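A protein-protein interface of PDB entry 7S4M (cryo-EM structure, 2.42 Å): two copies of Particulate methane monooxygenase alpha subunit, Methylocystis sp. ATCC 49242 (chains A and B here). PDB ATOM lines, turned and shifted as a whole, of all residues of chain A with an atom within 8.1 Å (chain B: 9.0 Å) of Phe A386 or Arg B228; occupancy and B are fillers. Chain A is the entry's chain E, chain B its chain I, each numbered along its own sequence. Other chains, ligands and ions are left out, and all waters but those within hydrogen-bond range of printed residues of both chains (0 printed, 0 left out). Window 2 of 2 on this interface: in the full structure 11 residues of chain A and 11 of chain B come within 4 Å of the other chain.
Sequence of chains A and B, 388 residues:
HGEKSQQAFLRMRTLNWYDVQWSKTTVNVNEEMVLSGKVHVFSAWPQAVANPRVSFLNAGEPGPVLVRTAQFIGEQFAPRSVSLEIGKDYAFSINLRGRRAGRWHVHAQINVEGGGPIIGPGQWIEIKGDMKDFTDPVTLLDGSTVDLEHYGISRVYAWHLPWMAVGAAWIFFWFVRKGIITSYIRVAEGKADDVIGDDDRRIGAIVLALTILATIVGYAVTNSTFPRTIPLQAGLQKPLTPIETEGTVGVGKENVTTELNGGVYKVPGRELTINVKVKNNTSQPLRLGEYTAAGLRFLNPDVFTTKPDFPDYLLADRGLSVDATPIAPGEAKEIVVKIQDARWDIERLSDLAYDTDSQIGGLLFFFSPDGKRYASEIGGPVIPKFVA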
ATOM      1  N   VAL A 264      22.043  11.623 -10.410  1.00  0.00           N
ATOM      2  CA  VAL A 264      21.678  11.585 -11.858  1.00  0.00           C
ATOM      3  C   VAL A 264      21.955  12.964 -12.459  1.00  0.00           C
ATOM      4  O   VAL A 264      21.368  13.943 -11.964  1.00  0.00           O
ATOM      5  CB  VAL A 264      20.215  11.141 -12.055  1.00  0.00           C
ATOM      6  CG1 VAL A 264      19.569  11.728 -13.300  1.00  0.00           C
ATOM      7  CG2 VAL A 264      20.075   9.626 -12.066  1.00  0.00           C
ATOM      8  N   TYR A 265      22.846  13.048 -13.451  1.00  0.00           N
ATOM      9  CA  TYR A 265      23.074  14.351 -14.136  1.00  0.00           C
ATOM     10  C   TYR A 265      22.632  14.234 -15.598  1.00  0.00           C
ATOM     11  O   TYR A 265      23.079  13.308 -16.296  1.00  0.00           O
ATOM     12  CB  TYR A 265      24.510  14.863 -13.960  1.00  0.00           C
ATOM     13  CG  TYR A 265      25.624  14.005 -14.497  1.00  0.00           C
ATOM     14  CD1 TYR A 265      26.087  12.915 -13.784  1.00  0.00           C
ATOM     15  CD2 TYR A 265      26.249  14.313 -15.694  1.00  0.00           C
ATOM     16  CE1 TYR A 265      27.121  12.130 -14.261  1.00  0.00           C
ATOM     17  CE2 TYR A 265      27.284  13.538 -16.186  1.00  0.00           C
ATOM     18  CZ  TYR A 265      27.723  12.445 -15.463  1.00  0.00           C
ATOM     19  OH  TYR A 265      28.737  11.663 -15.925  1.00  0.00           O
ATOM     20  N   LYS A 266      21.755  15.141 -16.035  1.00  0.00           N
ATOM     21  CA  LYS A 266      21.238  15.087 -17.427  1.00  0.00           C
ATOM     22  C   LYS A 266      22.358  15.476 -18.396  1.00  0.00           C
ATOM     23  O   LYS A 266      22.931  16.568 -18.220  1.00  0.00           O
ATOM     24  CB  LYS A 266      20.026  16.007 -17.583  1.00  0.00           C
ATOM     25  CG  LYS A 266      18.937  15.815 -16.540  1.00  0.00           C
ATOM     26  CD  LYS A 266      17.909  14.785 -16.934  1.00  0.00           C
ATOM     27  CE  LYS A 266      16.774  14.678 -15.938  1.00  0.00           C
ATOM     28  NZ  LYS A 266      17.216  14.054 -14.670  1.00  0.00           N
ATOM     29  N   VAL A 267      22.668  14.604 -19.357  1.00  0.00           N
ATOM     30  CA  VAL A 267      23.699  14.917 -20.391  1.00  0.00           C
ATOM     31  C   VAL A 267      23.043  14.803 -21.772  1.00  0.00           C
ATOM     32  O   VAL A 267      22.626  13.686 -22.131  1.00  0.00           O
ATOM     33  CB  VAL A 267      24.937  14.006 -20.282  1.00  0.00           C
ATOM     34  CG1 VAL A 267      26.157  14.780 -19.815  1.00  0.00           C
ATOM     35  CG2 VAL A 267      24.701  12.797 -19.395  1.00  0.00           C
ATOM     36  N   PRO A 268      22.939  15.893 -22.566  1.00  0.00           N
ATOM     37  CA  PRO A 268      23.275  17.245 -22.097  1.00  0.00           C
ATOM     38  C   PRO A 268      22.161  17.946 -21.301  1.00  0.00           C
ATOM     39  O   PRO A 268      20.998  17.752 -21.604  1.00  0.00           O
ATOM     40  CB  PRO A 268      23.533  18.005 -23.406  1.00  0.00           C
ATOM     41  CG  PRO A 268      22.660  17.312 -24.432  1.00  0.00           C
ATOM     42  CD  PRO A 268      22.544  15.872 -23.976  1.00  0.00           C
ATOM     43  N   ALA A 353      30.577  13.404 -17.854  1.00  0.00           N
ATOM     44  CA  ALA A 353      30.459  12.177 -18.634  1.00  0.00           C
ATOM     45  C   ALA A 353      31.719  11.905 -19.442  1.00  0.00           C
ATOM     46  O   ALA A 353      32.068  10.741 -19.669  1.00  0.00           O
ATOM     47  CB  ALA A 353      29.247  12.255 -19.558  1.00  0.00           C
ATOM     48  N   TYR A 354      32.409  12.954 -19.883  1.00  0.00           N
ATOM     49  CA  TYR A 354      33.642  12.779 -20.634  1.00  0.00           C
ATOM     50  C   TYR A 354      34.796  12.298 -19.766  1.00  0.00           C
ATOM     51  O   TYR A 354      35.769  11.755 -20.297  1.00  0.00           O
ATOM     52  CB  TYR A 354      34.020  14.090 -21.323  1.00  0.00           C
ATOM     53  CG  TYR A 354      35.273  14.007 -22.154  1.00  0.00           C
ATOM     54  CD1 TYR A 354      35.238  13.507 -23.446  1.00  0.00           C
ATOM     55  CD2 TYR A 354      36.495  14.436 -21.650  1.00  0.00           C
ATOM     56  CE1 TYR A 354      36.384  13.429 -24.211  1.00  0.00           C
ATOM     57  CE2 TYR A 354      37.644  14.361 -22.405  1.00  0.00           C
ATOM     58  CZ  TYR A 354      37.583  13.856 -23.684  1.00  0.00           C
ATOM     59  OH  TYR A 354      38.725  13.783 -24.446  1.00  0.00           O
ATOM     60  N   ILE A 383      25.515   8.800 -11.733  1.00  0.00           N
ATOM     61  CA  ILE A 383      25.165   8.084 -12.957  1.00  0.00           C
ATOM     62  C   ILE A 383      24.638   9.090 -13.969  1.00  0.00           C
ATOM     63  O   ILE A 383      23.686   9.816 -13.663  1.00  0.00           O
ATOM     64  CB  ILE A 383      24.122   6.983 -12.696  1.00  0.00           C
ATOM     65  CG1 ILE A 383      24.615   6.046 -11.597  1.00  0.00           C
ATOM     66  CG2 ILE A 383      23.841   6.215 -13.969  1.00  0.00           C
ATOM     67  CD1 ILE A 383      25.994   5.492 -11.847  1.00  0.00           C
ATOM     68  N   PRO A 384      25.204   9.211 -15.207  1.00  0.00           N
ATOM     69  CA  PRO A 384      24.637  10.104 -16.229  1.00  0.00           C
ATOM     70  C   PRO A 384      23.238   9.723 -16.729  1.00  0.00           C
ATOM     71  O   PRO A 384      22.933   8.546 -16.793  1.00  0.00           O
ATOM     72  CB  PRO A 384      25.586   9.994 -17.434  1.00  0.00           C
ATOM     73  CG  PRO A 384      26.284   8.686 -17.246  1.00  0.00           C
ATOM     74  CD  PRO A 384      26.459   8.622 -15.748  1.00  0.00           C
ATOM     75  N   LYS A 385      22.424  10.726 -17.057  1.00  0.00           N
ATOM     76  CA  LYS A 385      21.089  10.455 -17.647  1.00  0.00           C
ATOM     77  C   LYS A 385      21.144  10.932 -19.093  1.00  0.00           C
ATOM     78  O   LYS A 385      20.993  12.147 -19.322  1.00  0.00           O
ATOM     79  CB  LYS A 385      19.983  11.180 -16.879  1.00  0.00           C
ATOM     80  CG  LYS A 385      18.565  10.863 -17.337  1.00  0.00           C
ATOM     81  CD  LYS A 385      17.695  10.255 -16.258  1.00  0.00           C
ATOM     82  CE  LYS A 385      18.128   8.865 -15.843  1.00  0.00           C
ATOM     83  NZ  LYS A 385      18.198   7.938 -16.998  1.00  0.00           N
ATOM     84  N   PHE A 386      21.377  10.003 -20.020  1.00  0.00           N
ATOM     85  CA  PHE A 386      21.573  10.382 -21.443  1.00  0.00           C
ATOM     86  C   PHE A 386      20.271  10.885 -22.069  1.00  0.00           C
ATOM     87  O   PHE A 386      19.485  10.056 -22.563  1.00  0.00           O
ATOM     88  CB  PHE A 386      22.165   9.195 -22.205  1.00  0.00           C
ATOM     89  CG  PHE A 386      23.622   8.932 -21.920  1.00  0.00           C
ATOM     90  CD1 PHE A 386      24.544   9.965 -21.928  1.00  0.00           C
ATOM     91  CD2 PHE A 386      24.072   7.649 -21.648  1.00  0.00           C
ATOM     92  CE1 PHE A 386      25.885   9.723 -21.671  1.00  0.00           C
ATOM     93  CE2 PHE A 386      25.412   7.409 -21.391  1.00  0.00           C
ATOM     94  CZ  PHE A 386      26.316   8.446 -21.402  1.00  0.00           C
ATOM     95  N   VAL A 387      20.058  12.204 -22.055  1.00  0.00           N
ATOM     96  CA  VAL A 387      18.868  12.790 -22.741  1.00  0.00           C
ATOM     97  C   VAL A 387      19.159  12.786 -24.250  1.00  0.00           C
ATOM     98  O   VAL A 387      20.351  12.881 -24.631  1.00  0.00           O
ATOM     99  CB  VAL A 387      18.515  14.194 -22.198  1.00  0.00           C
ATOM    100  CG1 VAL A 387      19.128  14.464 -20.836  1.00  0.00           C
ATOM    101  CG2 VAL A 387      18.834  15.331 -23.157  1.00  0.00           C
ATOM    102  N   ALA A 388      18.121  12.637 -25.076  1.00  0.00           N
ATOM    103  CA  ALA A 388      18.310  12.637 -26.545  1.00  0.00           C
ATOM    104  C   ALA A 388      18.585  14.067 -27.028  1.00  0.00           C
ATOM    105  O   ALA A 388      19.769  14.374 -27.273  1.00  0.00           O
ATOM    106  CB  ALA A 388      17.101  12.040 -27.224  1.00  0.00           C
ATOM    107  N   LEU B 140      22.207  -2.440 -19.532  1.00  0.00           N
ATOM    108  CA  LEU B 140      22.821  -1.183 -19.925  1.00  0.00           C
ATOM    109  C   LEU B 140      22.107  -0.012 -19.263  1.00  0.00           C
ATOM    110  O   LEU B 140      21.083  -0.168 -18.595  1.00  0.00           O
ATOM    111  CB  LEU B 140      22.801  -1.034 -21.445  1.00  0.00           C
ATOM    112  CG  LEU B 140      24.043  -1.495 -22.207  1.00  0.00           C
ATOM    113  CD1 LEU B 140      24.466  -2.885 -21.780  1.00  0.00           C
ATOM    114  CD2 LEU B 140      23.780  -1.456 -23.699  1.00  0.00           C
ATOM    115  N   LEU B 141      22.670   1.184 -19.447  1.00  0.00           N
ATOM    116  CA  LEU B 141      22.038   2.380 -18.903  1.00  0.00           C
ATOM    117  C   LEU B 141      20.694   2.648 -19.561  1.00  0.00           C
ATOM    118  O   LEU B 141      19.753   3.089 -18.894  1.00  0.00           O
ATOM    119  CB  LEU B 141      22.957   3.587 -19.070  1.00  0.00           C
ATOM    120  CG  LEU B 141      23.850   3.912 -17.874  1.00  0.00           C
ATOM    121  CD1 LEU B 141      24.291   5.360 -17.930  1.00  0.00           C
ATOM    122  CD2 LEU B 141      23.132   3.615 -16.571  1.00  0.00           C
ATOM    123  N   ASP B 142      20.580   2.388 -20.864  1.00  0.00           N
ATOM    124  CA  ASP B 142      19.323   2.597 -21.567  1.00  0.00           C
ATOM    125  C   ASP B 142      18.252   1.589 -21.174  1.00  0.00           C
ATOM    126  O   ASP B 142      17.094   1.759 -21.566  1.00  0.00           O
ATOM    127  CB  ASP B 142      19.552   2.544 -23.077  1.00  0.00           C
ATOM    128  CG  ASP B 142      20.365   1.339 -23.502  1.00  0.00           C
ATOM    129  OD1 ASP B 142      20.032   0.214 -23.077  1.00  0.00           O
ATOM    130  OD2 ASP B 142      21.337   1.517 -24.263  1.00  0.00           O
ATOM    131  N   THR B 222      29.361   3.289 -37.019  1.00  0.00           N
ATOM    132  CA  THR B 222      29.455   2.870 -35.628  1.00  0.00           C
ATOM    133  C   THR B 222      29.290   4.029 -34.660  1.00  0.00           C
ATOM    134  O   THR B 222      29.370   3.813 -33.448  1.00  0.00           O
ATOM    135  CB  THR B 222      30.784   2.169 -35.357  1.00  0.00           C
ATOM    136  OG1 THR B 222      30.752   1.588 -34.050  1.00  0.00           O
ATOM    137  CG2 THR B 222      31.914   3.159 -35.410  1.00  0.00           C
ATOM    138  N   ASN B 223      29.095   5.246 -35.160  1.00  0.00           N
ATOM    139  CA  ASN B 223      28.692   6.354 -34.307  1.00  0.00           C
ATOM    140  C   ASN B 223      27.182   6.513 -34.256  1.00  0.00           C
ATOM    141  O   ASN B 223      26.651   6.969 -33.238  1.00  0.00           O
ATOM    142  CB  ASN B 223      29.332   7.657 -34.788  1.00  0.00           C
ATOM    143  CG  ASN B 223      30.450   8.119 -33.884  1.00  0.00           C
ATOM    144  OD1 ASN B 223      30.728   7.501 -32.859  1.00  0.00           O
ATOM    145  ND2 ASN B 223      31.102   9.210 -34.260  1.00  0.00           N
ATOM    146  N   SER B 224      26.482   6.160 -35.335  1.00  0.00           N
ATOM    147  CA  SER B 224      25.026   6.102 -35.283  1.00  0.00           C
ATOM    148  C   SER B 224      24.572   5.068 -34.264  1.00  0.00           C
ATOM    149  O   SER B 224      23.760   5.365 -33.382  1.00  0.00           O
ATOM    150  CB  SER B 224      24.463   5.786 -36.667  1.00  0.00           C
ATOM    151  OG  SER B 224      24.730   6.838 -37.574  1.00  0.00           O
ATOM    152  N   THR B 225      25.088   3.849 -34.372  1.00  0.00           N
ATOM    153  CA  THR B 225      24.980   2.901 -33.279  1.00  0.00           C
ATOM    154  C   THR B 225      25.886   3.351 -32.144  1.00  0.00           C
ATOM    155  O   THR B 225      26.934   3.956 -32.376  1.00  0.00           O
ATOM    156  CB  THR B 225      25.372   1.502 -33.742  1.00  0.00           C
ATOM    157  OG1 THR B 225      24.920   1.302 -35.086  1.00  0.00           O
ATOM    158  CG2 THR B 225      24.740   0.455 -32.849  1.00  0.00           C
ATOM    159  N   PHE B 226      25.477   3.060 -30.913  1.00  0.00           N
ATOM    160  CA  PHE B 226      26.190   3.502 -29.720  1.00  0.00           C
ATOM    161  C   PHE B 226      26.517   4.996 -29.785  1.00  0.00           C
ATOM    162  O   PHE B 226      27.690   5.383 -29.729  1.00  0.00           O
ATOM    163  CB  PHE B 226      27.458   2.685 -29.512  1.00  0.00           C
ATOM    164  CG  PHE B 226      27.367   1.283 -30.026  1.00  0.00           C
ATOM    165  CD1 PHE B 226      26.504   0.377 -29.446  1.00  0.00           C
ATOM    166  CD2 PHE B 226      28.152   0.869 -31.082  1.00  0.00           C
ATOM    167  CE1 PHE B 226      26.420  -0.914 -29.914  1.00  0.00           C
ATOM    168  CE2 PHE B 226      28.076  -0.423 -31.553  1.00  0.00           C
ATOM    169  CZ  PHE B 226      27.208  -1.314 -30.969  1.00  0.00           C
ATOM    170  N   PRO B 227      25.508   5.861 -29.917  1.00  0.00           N
ATOM    171  CA  PRO B 227      25.792   7.298 -30.013  1.00  0.00           C
ATOM    172  C   PRO B 227      26.276   7.907 -28.712  1.00  0.00           C
ATOM    173  O   PRO B 227      26.841   9.008 -28.738  1.00  0.00           O
ATOM    174  CB  PRO B 227      24.444   7.892 -30.428  1.00  0.00           C
ATOM    175  CG  PRO B 227      23.445   6.966 -29.847  1.00  0.00           C
ATOM    176  CD  PRO B 227      24.063   5.593 -29.816  1.00  0.00           C
ATOM    177  N   ARG B 228      26.075   7.236 -27.582  1.00  0.00           N
ATOM    178  CA  ARG B 228      26.462   7.753 -26.271  1.00  0.00           C
ATOM    179  C   ARG B 228      27.359   6.718 -25.603  1.00  0.00           C
ATOM    180  O   ARG B 228      26.874   5.712 -25.079  1.00  0.00           O
ATOM    181  CB  ARG B 228      25.235   8.060 -25.423  1.00  0.00           C
ATOM    182  CG  ARG B 228      24.085   8.651 -26.216  1.00  0.00           C
ATOM    183  CD  ARG B 228      23.478   9.848 -25.512  1.00  0.00           C
ATOM    184  NE  ARG B 228      24.378  10.993 -25.492  1.00  0.00           N
ATOM    185  CZ  ARG B 228      24.654  11.754 -26.543  1.00  0.00           C
ATOM    186  NH1 ARG B 228      24.102  11.527 -27.724  1.00  0.00           N
ATOM    187  NH2 ARG B 228      25.499  12.771 -26.404  1.00  0.00           N
ATOM    188  N   THR B 229      28.662   6.967 -25.626  1.00  0.00           N
ATOM    189  CA  THR B 229      29.643   6.097 -25.005  1.00  0.00           C
ATOM    190  C   THR B 229      30.453   6.893 -23.993  1.00  0.00           C
ATOM    191  O   THR B 229      30.490   8.125 -24.027  1.00  0.00           O
ATOM    192  CB  THR B 229      30.578   5.476 -26.046  1.00  0.00           C
ATOM    193  OG1 THR B 229      31.220   6.516 -26.791  1.00  0.00           O
ATOM    194  CG2 THR B 229      29.798   4.589 -26.998  1.00  0.00           C
ATOM    195  N   ILE B 230      31.101   6.176 -23.084  1.00  0.00           N
ATOM    196  CA  ILE B 230      31.880   6.820 -22.031  1.00  0.00           C
ATOM    197  C   ILE B 230      33.286   6.237 -22.019  1.00  0.00           C
ATOM    198  O   ILE B 230      33.484   5.087 -22.434  1.00  0.00           O
ATOM    199  CB  ILE B 230      31.203   6.654 -20.664  1.00  0.00           C
ATOM    200  CG1 ILE B 230      30.854   5.191 -20.421  1.00  0.00           C
ATOM    201  CG2 ILE B 230      29.957   7.513 -20.585  1.00  0.00           C
ATOM    202  CD1 ILE B 230      30.806   4.825 -18.966  1.00  0.00           C
ATOM    203  N   PRO B 231      34.287   6.985 -21.570  1.00  0.00           N
ATOM    204  CA  PRO B 231      35.639   6.431 -21.478  1.00  0.00           C
ATOM    205  C   PRO B 231      35.741   5.402 -20.367  1.00  0.00           C
ATOM    206  O   PRO B 231      34.887   5.311 -19.484  1.00  0.00           O
ATOM    207  CB  PRO B 231      36.505   7.656 -21.178  1.00  0.00           C
ATOM    208  CG  PRO B 231      35.573   8.618 -20.541  1.00  0.00           C
ATOM    209  CD  PRO B 231      34.251   8.410 -21.204  1.00  0.00           C
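OH of Tyr A265 is in hydrogen-bond range of N of Ala A353 (3.2 Å).
The backbone carbonyl oxygen (O) of Ile A383 is in hydrogen-bond range of the backbone NH (N) of Tyr A265, at 3.3 Å.
Ala A353 touches Ile B230.
Ala A353 touches Pro B231 (O to CD, 3.5 Å).
Tyr A354 touches Pro B231 (O to CG, 3.2 Å).
CG2 of Ile A383 touches CD2 of Leu B141, 3.7 Å away.
Pro A384 touches Leu B141.
Arg B228 touches Phe A386 (CD to CB, 3.6 Å).
CZ of Phe A386 touches CG2 of Ile B230 (3.8 Å).
Of the printed residues of chain B, Tyr A354 touches Pro B231 (3.2 Å).
Of the printed residues of chain B, Ile A383 touches Leu B141 (3.7 Å).
Of chain B, only Arg B228 (3.6 Å) and Ile B230 (3.8 Å) come within 4 Å of Phe A386.
No residue of chain B comes within 4 Å of Val A387.
Printed residues of chain A within 4 Å of Leu B141: Ile A383 (3.7 Å) and Pro A384 (3.6 Å).
Ser B224 touches none of the printed residues of chain A.
Of chain A, only Phe A386 comes within 4 Å of Arg B228.
No residue of chain A comes within 4 Å of Thr B229.
Of the printed residues of chain A, Ile B230 touches Ala A353 (3.96 Å) and Phe A386 (3.8 Å).
Printed residues of chain A within 4 Å of Pro B231: Ala A353 and Tyr A354.
The nearest residue of chain A that does not touch Arg B228 is Val A387 (4.4 Å).
The nearest printed residue of chain B that does not touch Tyr A354 is Ile B230 (6.0 Å).
Of the 13 printed residues of chain A, 5 touch a printed residue of chain B.
Hydrophobic or aromatic side chains of chain A within 4 Å of the printed part of chain B: Ile A383, Pro A384 and Phe A386.
Of the 13 printed residues of chain B, 4 touch a printed residue of chain A.
Hydrophobic or aromatic side chains of chain B that line the printed part of chain A: Leu B141, Ile B230 and Pro B231.
Among the printed residues, 7 pairs touch across the chains.
Among the printed residues, no Asp or Glu carboxylate lies within 4 Å of a Lys or Arg side-chain nitrogen of the other chain.
No position is printed for both chains.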
